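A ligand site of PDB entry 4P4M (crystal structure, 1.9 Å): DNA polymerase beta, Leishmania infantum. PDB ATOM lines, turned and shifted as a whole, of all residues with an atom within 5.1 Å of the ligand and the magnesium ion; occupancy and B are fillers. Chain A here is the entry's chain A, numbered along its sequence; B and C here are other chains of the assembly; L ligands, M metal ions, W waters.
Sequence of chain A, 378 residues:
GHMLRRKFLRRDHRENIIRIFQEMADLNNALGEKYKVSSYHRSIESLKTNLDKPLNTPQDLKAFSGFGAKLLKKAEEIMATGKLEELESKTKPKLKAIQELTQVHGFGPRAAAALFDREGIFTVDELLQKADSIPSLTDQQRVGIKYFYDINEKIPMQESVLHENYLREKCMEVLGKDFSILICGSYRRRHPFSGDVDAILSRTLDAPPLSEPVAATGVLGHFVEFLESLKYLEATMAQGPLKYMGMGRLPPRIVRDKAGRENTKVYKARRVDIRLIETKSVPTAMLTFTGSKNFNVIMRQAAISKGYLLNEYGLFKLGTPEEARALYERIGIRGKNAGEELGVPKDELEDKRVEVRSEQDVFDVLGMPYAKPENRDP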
ATOM      1  N   GLY A 185      -6.144 -17.613  19.645  1.00  0.00           N
ATOM      2  CA  GLY A 185      -6.374 -17.604  18.203  1.00  0.00           C
ATOM      3  C   GLY A 185      -6.093 -16.269  17.522  1.00  0.00           C
ATOM      4  O   GLY A 185      -5.356 -15.427  18.047  1.00  0.00           O
ATOM      5  N   SER A 186      -6.670 -16.066  16.340  1.00  0.00           N
ATOM      6  CA  SER A 186      -6.430 -14.856  15.559  1.00  0.00           C
ATOM      7  C   SER A 186      -7.001 -13.583  16.211  1.00  0.00           C
ATOM      8  O   SER A 186      -6.566 -12.472  15.903  1.00  0.00           O
ATOM      9  CB  SER A 186      -6.970 -15.003  14.129  1.00  0.00           C
ATOM     10  OG  SER A 186      -8.364 -15.256  14.151  1.00  0.00           O
ATOM     11  N   ARG A 189      -4.269 -12.281  18.181  1.00  0.00           N
ATOM     12  CA  ARG A 189      -3.345 -11.695  17.205  1.00  0.00           C
ATOM     13  C   ARG A 189      -3.903 -10.395  16.590  1.00  0.00           C
ATOM     14  O   ARG A 189      -3.305  -9.807  15.679  1.00  0.00           O
ATOM     15  CB  ARG A 189      -2.984 -12.715  16.099  1.00  0.00           C
ATOM     16  CG  ARG A 189      -2.338 -14.016  16.640  1.00  0.00           C
ATOM     17  CD  ARG A 189      -1.453 -14.759  15.597  1.00  0.00           C
ATOM     18  NE  ARG A 189      -2.097 -14.960  14.295  1.00  0.00           N
ATOM     19  CZ  ARG A 189      -2.998 -15.904  14.025  1.00  0.00           C
ATOM     20  NH1 ARG A 189      -3.405 -16.741  14.976  1.00  0.00           N
ATOM     21  NH2 ARG A 189      -3.502 -15.990  12.803  1.00  0.00           N
ATOM     22  N   PHE A 193     -11.111  -9.850  11.825  1.00  0.00           N
ATOM     23  CA  PHE A 193     -12.055 -10.962  11.778  1.00  0.00           C
ATOM     24  C   PHE A 193     -11.387 -12.274  12.190  1.00  0.00           C
ATOM     25  O   PHE A 193     -10.169 -12.432  12.014  1.00  0.00           O
ATOM     26  CB  PHE A 193     -12.652 -11.124  10.377  1.00  0.00           C
ATOM     27  CG  PHE A 193     -13.391  -9.906   9.891  1.00  0.00           C
ATOM     28  CD1 PHE A 193     -14.733  -9.731  10.195  1.00  0.00           C
ATOM     29  CD2 PHE A 193     -12.737  -8.932   9.157  1.00  0.00           C
ATOM     30  CE1 PHE A 193     -15.420  -8.598   9.764  1.00  0.00           C
ATOM     31  CE2 PHE A 193     -13.415  -7.805   8.717  1.00  0.00           C
ATOM     32  CZ  PHE A 193     -14.749  -7.637   9.023  1.00  0.00           C
ATOM     33  N   SER A 194     -12.169 -13.216  12.704  1.00  0.00           N
ATOM     34  CA  SER A 194     -11.665 -14.540  13.070  1.00  0.00           C
ATOM     35  C   SER A 194     -12.621 -15.631  12.571  1.00  0.00           C
ATOM     36  O   SER A 194     -13.822 -15.409  12.447  1.00  0.00           O
ATOM     37  CB  SER A 194     -11.506 -14.666  14.580  1.00  0.00           C
ATOM     38  OG  SER A 194     -10.456 -13.851  15.076  1.00  0.00           O
ATOM     39  N   GLY A 195     -12.072 -16.818  12.322  1.00  0.00           N
ATOM     40  CA  GLY A 195     -12.881 -17.933  11.852  1.00  0.00           C
ATOM     41  C   GLY A 195     -13.696 -18.603  12.956  1.00  0.00           C
ATOM     42  O   GLY A 195     -14.807 -19.049  12.714  1.00  0.00           O
ATOM     43  N   ASP A 196     -13.126 -18.673  14.159  1.00  0.00           N
ATOM     44  CA  ASP A 196     -13.777 -19.366  15.286  1.00  0.00           C
ATOM     45  C   ASP A 196     -13.398 -18.671  16.603  1.00  0.00           C
ATOM     46  O   ASP A 196     -12.751 -17.617  16.603  1.00  0.00           O
ATOM     47  CB  ASP A 196     -13.409 -20.856  15.301  1.00  0.00           C
ATOM     48  CG  ASP A 196     -12.002 -21.124  15.864  1.00  0.00           C
ATOM     49  OD1 ASP A 196     -11.173 -20.203  15.840  1.00  0.00           O
ATOM     50  OD2 ASP A 196     -11.719 -22.240  16.344  1.00  0.00           O
ATOM     51  N   ASP A 198     -11.293 -19.501  20.006  1.00  0.00           N
ATOM     52  CA  ASP A 198     -10.369 -20.435  20.647  1.00  0.00           C
ATOM     53  C   ASP A 198     -10.158 -20.078  22.117  1.00  0.00           C
ATOM     54  O   ASP A 198      -9.480 -19.092  22.435  1.00  0.00           O
ATOM     55  CB  ASP A 198      -8.997 -20.425  19.944  1.00  0.00           C
ATOM     56  CG  ASP A 198      -9.090 -20.815  18.476  1.00  0.00           C
ATOM     57  OD1 ASP A 198      -9.505 -21.955  18.170  1.00  0.00           O
ATOM     58  OD2 ASP A 198      -8.735 -19.974  17.627  1.00  0.00           O
ATOM     59  N   THR A 288       0.779 -21.844  21.950  1.00  0.00           N
ATOM     60  CA  THR A 288       0.227 -22.805  20.984  1.00  0.00           C
ATOM     61  C   THR A 288      -1.108 -22.332  20.422  1.00  0.00           C
ATOM     62  O   THR A 288      -1.319 -22.343  19.197  1.00  0.00           O
ATOM     63  CB  THR A 288       0.025 -24.209  21.624  1.00  0.00           C
ATOM     64  OG1 THR A 288       1.301 -24.796  21.896  1.00  0.00           O
ATOM     65  CG2 THR A 288      -0.752 -25.120  20.675  1.00  0.00           C
ATOM     66  N   PHE A 289      -2.020 -21.937  21.308  1.00  0.00           N
ATOM     67  CA  PHE A 289      -3.381 -21.649  20.828  1.00  0.00           C
ATOM     68  C   PHE A 289      -3.546 -20.246  20.243  1.00  0.00           C
ATOM     69  O   PHE A 289      -4.548 -19.953  19.614  1.00  0.00           O
ATOM     70  CB  PHE A 289      -4.441 -22.011  21.886  1.00  0.00           C
ATOM     71  CG  PHE A 289      -4.401 -23.469  22.265  1.00  0.00           C
ATOM     72  CD1 PHE A 289      -4.641 -24.438  21.302  1.00  0.00           C
ATOM     73  CD2 PHE A 289      -4.093 -23.859  23.549  1.00  0.00           C
ATOM     74  CE1 PHE A 289      -4.581 -25.790  21.622  1.00  0.00           C
ATOM     75  CE2 PHE A 289      -4.029 -25.205  23.881  1.00  0.00           C
ATOM     76  CZ  PHE A 289      -4.277 -26.167  22.917  1.00  0.00           C
ATOM     77  N   THR A 290      -2.538 -19.407  20.425  1.00  0.00           N
ATOM     78  CA  THR A 290      -2.467 -18.118  19.727  1.00  0.00           C
ATOM     79  C   THR A 290      -1.944 -18.284  18.285  1.00  0.00           C
ATOM     80  O   THR A 290      -2.431 -17.628  17.365  1.00  0.00           O
ATOM     81  CB  THR A 290      -1.623 -17.078  20.526  1.00  0.00           C
ATOM     82  OG1 THR A 290      -2.245 -16.838  21.799  1.00  0.00           O
ATOM     83  CG2 THR A 290      -1.543 -15.727  19.763  1.00  0.00           C
ATOM     84  N   GLY A 291      -0.969 -19.174  18.079  1.00  0.00           N
ATOM     85  CA  GLY A 291      -0.463 -19.390  16.733  1.00  0.00           C
ATOM     86  C   GLY A 291       0.256 -18.159  16.177  1.00  0.00           C
ATOM     87  O   GLY A 291       0.834 -17.398  16.959  1.00  0.00           O
ATOM     88  N   SER A 292       0.234 -17.934  14.869  1.00  0.00           N
ATOM     89  CA  SER A 292      -0.468 -18.736  13.873  1.00  0.00           C
ATOM     90  C   SER A 292       0.068 -20.161  13.765  1.00  0.00           C
ATOM     91  O   SER A 292       1.066 -20.519  14.399  1.00  0.00           O
ATOM     92  CB  SER A 292      -0.294 -18.083  12.488  1.00  0.00           C
ATOM     93  OG  SER A 292       1.054 -18.256  12.052  1.00  0.00           O
ATOM     94  N   LYS A 293      -0.593 -20.963  12.943  1.00  0.00           N
ATOM     95  CA  LYS A 293      -0.107 -22.309  12.636  1.00  0.00           C
ATOM     96  C   LYS A 293       1.347 -22.320  12.164  1.00  0.00           C
ATOM     97  O   LYS A 293       2.174 -23.097  12.664  1.00  0.00           O
ATOM     98  CB  LYS A 293      -0.995 -22.981  11.582  1.00  0.00           C
ATOM     99  CG  LYS A 293      -0.439 -24.298  11.046  1.00  0.00           C
ATOM    100  CD  LYS A 293      -1.177 -24.723   9.787  1.00  0.00           C
ATOM    101  CE  LYS A 293      -0.757 -26.107   9.330  1.00  0.00           C
ATOM    102  NZ  LYS A 293       0.693 -26.178   8.996  1.00  0.00           N
ATOM    103  N   ASN A 296       3.837 -21.562  14.961  1.00  0.00           N
ATOM    104  CA  ASN A 296       4.061 -22.710  15.856  1.00  0.00           C
ATOM    105  C   ASN A 296       5.032 -23.715  15.239  1.00  0.00           C
ATOM    106  O   ASN A 296       5.872 -24.276  15.935  1.00  0.00           O
ATOM    107  CB  ASN A 296       2.738 -23.446  16.181  1.00  0.00           C
ATOM    108  CG  ASN A 296       1.812 -22.633  17.088  1.00  0.00           C
ATOM    109  OD1 ASN A 296       2.201 -21.618  17.655  1.00  0.00           O
ATOM    110  ND2 ASN A 296       0.580 -23.123  17.247  1.00  0.00           N
ATOM    111  N   ARG A 300       8.546 -24.628  16.903  1.00  0.00           N
ATOM    112  CA  ARG A 300       8.804 -26.023  17.262  1.00  0.00           C
ATOM    113  C   ARG A 300      10.041 -26.586  16.544  1.00  0.00           C
ATOM    114  O   ARG A 300      10.768 -27.424  17.090  1.00  0.00           O
ATOM    115  CB  ARG A 300       7.542 -26.888  17.025  1.00  0.00           C
ATOM    116  CG  ARG A 300       6.413 -26.525  18.016  1.00  0.00           C
ATOM    117  CD  ARG A 300       5.028 -27.079  17.635  1.00  0.00           C
ATOM    118  NE  ARG A 300       4.056 -26.683  18.661  1.00  0.00           N
ATOM    119  CZ  ARG A 300       2.920 -27.326  18.900  1.00  0.00           C
ATOM    120  NH1 ARG A 300       2.569 -28.384  18.173  1.00  0.00           N
ATOM    121  NH2 ARG A 300       2.115 -26.899  19.883  1.00  0.00           N
ATOM    122  OP3  DA B   1       9.435 -31.238  10.663  1.00  0.00           O
ATOM    123  P    DA B   1       8.030 -30.772  10.558  1.00  0.00           P
ATOM    124  OP1  DA B   1       7.198 -31.950  10.252  1.00  0.00           O
ATOM    125  OP2  DA B   1       8.024 -29.605   9.659  1.00  0.00           O
ATOM    126  O5'  DA B   1       7.557 -30.259  11.987  1.00  0.00           O
ATOM    127  C5'  DA B   1       8.357 -29.423  12.791  1.00  0.00           C
ATOM    128  C4'  DA B   1       7.775 -29.452  14.204  1.00  0.00           C
ATOM    129  O4'  DA B   1       6.452 -28.863  14.177  1.00  0.00           O
ATOM    130  C3'  DA B   1       7.615 -30.843  14.813  1.00  0.00           C
ATOM    131  O3'  DA B   1       7.933 -30.712  16.204  1.00  0.00           O
ATOM    132  C2'  DA B   1       6.137 -31.162  14.544  1.00  0.00           C
ATOM    133  C1'  DA B   1       5.469 -29.789  14.610  1.00  0.00           C
ATOM    134  N9   DA B   1       4.289 -29.631  13.747  1.00  0.00           N
ATOM    135  C8   DA B   1       4.169 -30.084  12.453  1.00  0.00           C
ATOM    136  N7   DA B   1       3.021 -29.794  11.895  1.00  0.00           N
ATOM    137  C5   DA B   1       2.328 -29.101  12.873  1.00  0.00           C
ATOM    138  C6   DA B   1       1.037 -28.518  12.873  1.00  0.00           C
ATOM    139  N6   DA B   1       0.204 -28.574  11.820  1.00  0.00           N
ATOM    140  N1   DA B   1       0.642 -27.886  14.001  1.00  0.00           N
ATOM    141  C2   DA B   1       1.485 -27.851  15.045  1.00  0.00           C
ATOM    142  N3   DA B   1       2.717 -28.361  15.161  1.00  0.00           N
ATOM    143  C4   DA B   1       3.099 -28.979  14.021  1.00  0.00           C
ATOM    144  P    DT B   2       8.055 -32.000  17.148  1.00  0.00           P
ATOM    145  OP1  DT B   2       8.976 -31.664  18.263  1.00  0.00           O
ATOM    146  OP2  DT B   2       8.324 -33.180  16.286  1.00  0.00           O
ATOM    147  O5'  DT B   2       6.585 -32.175  17.724  1.00  0.00           O
ATOM    148  C5'  DT B   2       6.085 -31.181  18.614  1.00  0.00           C
ATOM    149  C4'  DT B   2       4.595 -31.382  18.794  1.00  0.00           C
ATOM    150  O4'  DT B   2       3.895 -31.051  17.565  1.00  0.00           O
ATOM    151  C3'  DT B   2       4.152 -32.797  19.177  1.00  0.00           C
ATOM    152  O3'  DT B   2       3.772 -32.750  20.567  1.00  0.00           O
ATOM    153  C2'  DT B   2       2.969 -33.084  18.245  1.00  0.00           C
ATOM    154  C1'  DT B   2       2.647 -31.708  17.656  1.00  0.00           C
ATOM    155  N1   DT B   2       1.946 -31.748  16.325  1.00  0.00           N
ATOM    156  C2   DT B   2       0.755 -31.056  16.191  1.00  0.00           C
ATOM    157  O2   DT B   2       0.237 -30.405  17.079  1.00  0.00           O
ATOM    158  N3   DT B   2       0.167 -31.149  14.961  1.00  0.00           N
ATOM    159  C4   DT B   2       0.637 -31.841  13.875  1.00  0.00           C
ATOM    160  O4   DT B   2       0.013 -31.856  12.818  1.00  0.00           O
ATOM    161  C5   DT B   2       1.890 -32.546  14.061  1.00  0.00           C
ATOM    162  C7   DT B   2       2.486 -33.345  12.931  1.00  0.00           C
ATOM    163  C6   DT B   2       2.477 -32.472  15.269  1.00  0.00           C
ATOM    164  P    DA C   5     -11.203 -26.993  13.338  1.00  0.00           P
ATOM    165  OP1  DA C   5     -12.390 -26.270  13.844  1.00  0.00           O
ATOM    166  OP2  DA C   5     -10.443 -26.405  12.215  1.00  0.00           O
ATOM    167  O5'  DA C   5     -10.249 -27.245  14.576  1.00  0.00           O
ATOM    168  C5'  DA C   5      -9.576 -26.210  15.226  1.00  0.00           C
ATOM    169  C4'  DA C   5      -8.878 -26.775  16.444  1.00  0.00           C
ATOM    170  O4'  DA C   5      -8.044 -27.900  16.066  1.00  0.00           O
ATOM    171  C3'  DA C   5      -7.929 -25.764  17.069  1.00  0.00           C
ATOM    172  O3'  DA C   5      -7.682 -26.101  18.447  1.00  0.00           O
ATOM    173  C2'  DA C   5      -6.707 -25.960  16.162  1.00  0.00           C
ATOM    174  C1'  DA C   5      -6.676 -27.483  16.104  1.00  0.00           C
ATOM    175  N9   DA C   5      -5.931 -28.106  14.999  1.00  0.00           N
ATOM    176  C8   DA C   5      -6.308 -28.276  13.695  1.00  0.00           C
ATOM    177  N7   DA C   5      -5.432 -28.919  12.955  1.00  0.00           N
ATOM    178  C5   DA C   5      -4.393 -29.190  13.840  1.00  0.00           C
ATOM    179  C6   DA C   5      -3.149 -29.852  13.689  1.00  0.00           C
ATOM    180  N6   DA C   5      -2.700 -30.378  12.541  1.00  0.00           N
ATOM    181  N1   DA C   5      -2.350 -29.952  14.784  1.00  0.00           N
ATOM    182  C2   DA C   5      -2.792 -29.432  15.934  1.00  0.00           C
ATOM    183  N3   DA C   5      -3.935 -28.789  16.196  1.00  0.00           N
ATOM    184  C4   DA C   5      -4.696 -28.708  15.098  1.00  0.00           C
HETATM  185  P1  LIG L   1      -7.237 -21.830  14.056  1.00  0.00           P
HETATM  186  O1  LIG L   1      -8.480 -21.571  14.840  1.00  0.00           O
HETATM  187  O2  LIG L   1      -7.339 -22.978  13.088  1.00  0.00           O
HETATM  188  O3  LIG L   1      -6.422 -22.738  15.353  1.00  0.00           O
HETATM  189  C1  LIG L   1      -6.187 -22.042  16.467  1.00  0.00           C
HETATM  190  C2  LIG L   1      -4.701 -22.213  16.962  1.00  0.00           C
HETATM  191  O4  LIG L   1      -4.310 -23.593  16.940  1.00  0.00           O
HETATM  192  C3  LIG L   1      -2.980 -23.700  16.567  1.00  0.00           C
HETATM  193  N1  LIG L   1      -2.863 -24.654  15.425  1.00  0.00           N
HETATM  194  C4  LIG L   1      -3.790 -24.599  14.402  1.00  0.00           C
HETATM  195  C5  LIG L   1      -1.744 -25.583  15.370  1.00  0.00           C
HETATM  196  O5  LIG L   1      -0.923 -25.631  16.247  1.00  0.00           O
HETATM  197  N2  LIG L   1      -1.671 -26.434  14.227  1.00  0.00           N
HETATM  198  C6  LIG L   1      -2.608 -26.329  13.298  1.00  0.00           C
HETATM  199  O6  LIG L   1      -2.504 -27.147  12.237  1.00  0.00           O
HETATM  200  C7  LIG L   1      -3.718 -25.431  13.292  1.00  0.00           C
HETATM  201  C8  LIG L   1      -4.672 -25.436  12.176  1.00  0.00           C
HETATM  202  C9  LIG L   1      -2.452 -22.316  16.138  1.00  0.00           C
HETATM  203  C10 LIG L   1      -3.723 -21.502  15.998  1.00  0.00           C
HETATM  204  O7  LIG L   1      -6.127 -20.766  13.858  1.00  0.00           O
HETATM  205  P2  LIG L   1      -6.482 -19.055  13.874  1.00  0.00           P
HETATM  206  O8  LIG L   1      -7.131 -18.943  15.212  1.00  0.00           O
HETATM  207  O9  LIG L   1      -5.043 -18.647  13.823  1.00  0.00           O
HETATM  208  O10 LIG L   1      -7.310 -18.526  12.696  1.00  0.00           O
HETATM  209  P3  LIG L   1      -8.984 -18.390  12.373  1.00  0.00           P
HETATM  210  O11 LIG L   1      -9.711 -18.978  13.544  1.00  0.00           O
HETATM  211  O12 LIG L   1      -9.138 -19.218  11.102  1.00  0.00           O
HETATM  212  O13 LIG L   1      -9.209 -16.907  12.234  1.00  0.00           O
HETATM  213 MG    MG M   1      -9.126 -19.610  15.534  1.00  0.00          MG
HETATM  214  O   HOH W   1      -9.831 -17.582  16.312  1.00  0.00           O
HETATM  215  O   HOH W   2      -7.152 -20.175   9.710  1.00  0.00           O
HETATM  216  O   HOH W   3      -3.248 -27.740   9.599  1.00  0.00           O
HETATM  217  O   HOH W   4      -3.357 -20.035  12.188  1.00  0.00           O
HETATM  218  O   HOH W   5      -1.351 -27.399  18.245  1.00  0.00           O
HETATM  219  O   HOH W   6     -10.513 -21.630  11.973  1.00  0.00           O
HETATM  220  O   HOH W   7      -8.763 -15.838  10.059  1.00  0.00           O
HETATM  221  O   HOH W   8      -5.460 -16.698  10.616  1.00  0.00           O
HETATM  222  O   HOH W   9     -10.652 -19.274   9.013  1.00  0.00           O
HETATM  223  O   HOH W  10      -5.002 -22.137  11.202  1.00  0.00           O
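The side-chain hydroxyl (OG) of Ser 194 sits at hydrogen-bond distance from the side-chain hydroxyl (OG) of Ser 186 (2.7 Å).
The guanidinium group (NH1) of Arg 300 is in hydrogen-bond range of N3 of DA 1 of chain B (3.0 Å).
NH1 of Arg 189 is in hydrogen-bond range of O of Thr 290 (2.7 Å).
ND2 of Asn 296 is in hydrogen-bond range of O of Thr 288, 2.8 Å away.
The side-chain hydroxyl (OG1) of Thr 288 sits at hydrogen-bond distance from the guanidinium group (NH2) of Arg 300.
O of Phe 289 is in hydrogen-bond range of N of Gly 185 (2.8 Å).
N6 of DA 5 of chain C lies close to an oxygen (O6) of the ligand, at 3.3 Å.
Gly 185 touches the ligand (CA to O8, 3.4 Å).
Ser 194 touches the ligand.
Thr 288 touches the ligand (O to C9, 3.3 Å).
O of Phe 289 touches C2 of the ligand, at 3.5 Å.
Gly 291 touches the ligand (CA to C9, 3.6 Å).
CE of Lys 293 touches O6 of the ligand (3.5 Å).
Water W1 bridges O of Asp 196 and OG of Ser 186.
Water W4 bridges an oxygen (O9) of the ligand and the backbone NH of Lys 293.
Water W8 lies within hydrogen-bond range of NH2 of Arg 189 (3.0 Å) and O10 of the ligand (3.3 Å).
An oxygen (O8) of the ligand is bound to the magnesium ion (2.1 Å).
The magnesium ion is bound by OD1 of Asp 196, at 2.2 Å.
The side-chain carboxylate (OD2) of Asp 198 is bound to the magnesium ion (2.2 Å).
The magnesium ion is bound by an oxygen (O11) of the ligand, at 2.2 Å.
O1 of the ligand is bound to the magnesium ion.
Water W1 binds the magnesium ion, at 2.3 Å.
Two residues have an atom within 4 Å of the magnesium ion: Asp 196 and Asp 198.
The nearest printed residue that does not touch the magnesium ion is Gly 185 (4.3 Å).
An oxygen (O11) of the ligand lies close to the backbone NH (N) of Asp 196 (3.5 Å).
The backbone NH (N) of Ser 186 lies close to an oxygen (O8) of the ligand (3.1 Å).
An oxygen (O13) of the ligand lies within hydrogen-bond range of the side-chain hydroxyl of Ser 186 (2.7 Å).
N1 of DA 1 of chain B sits at hydrogen-bond distance from N2 of the ligand (2.7 Å).
NH1 of Arg 189 is in salt-bridge range of O9 of the ligand, at 2.8 Å.
O13 of the ligand is in hydrogen-bond range of N of Gly 195, at 2.9 Å.
An oxygen (O5) of the ligand lies within hydrogen-bond range of the side-chain amide nitrogen (ND2) of Asn 296, 3.1 Å away.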
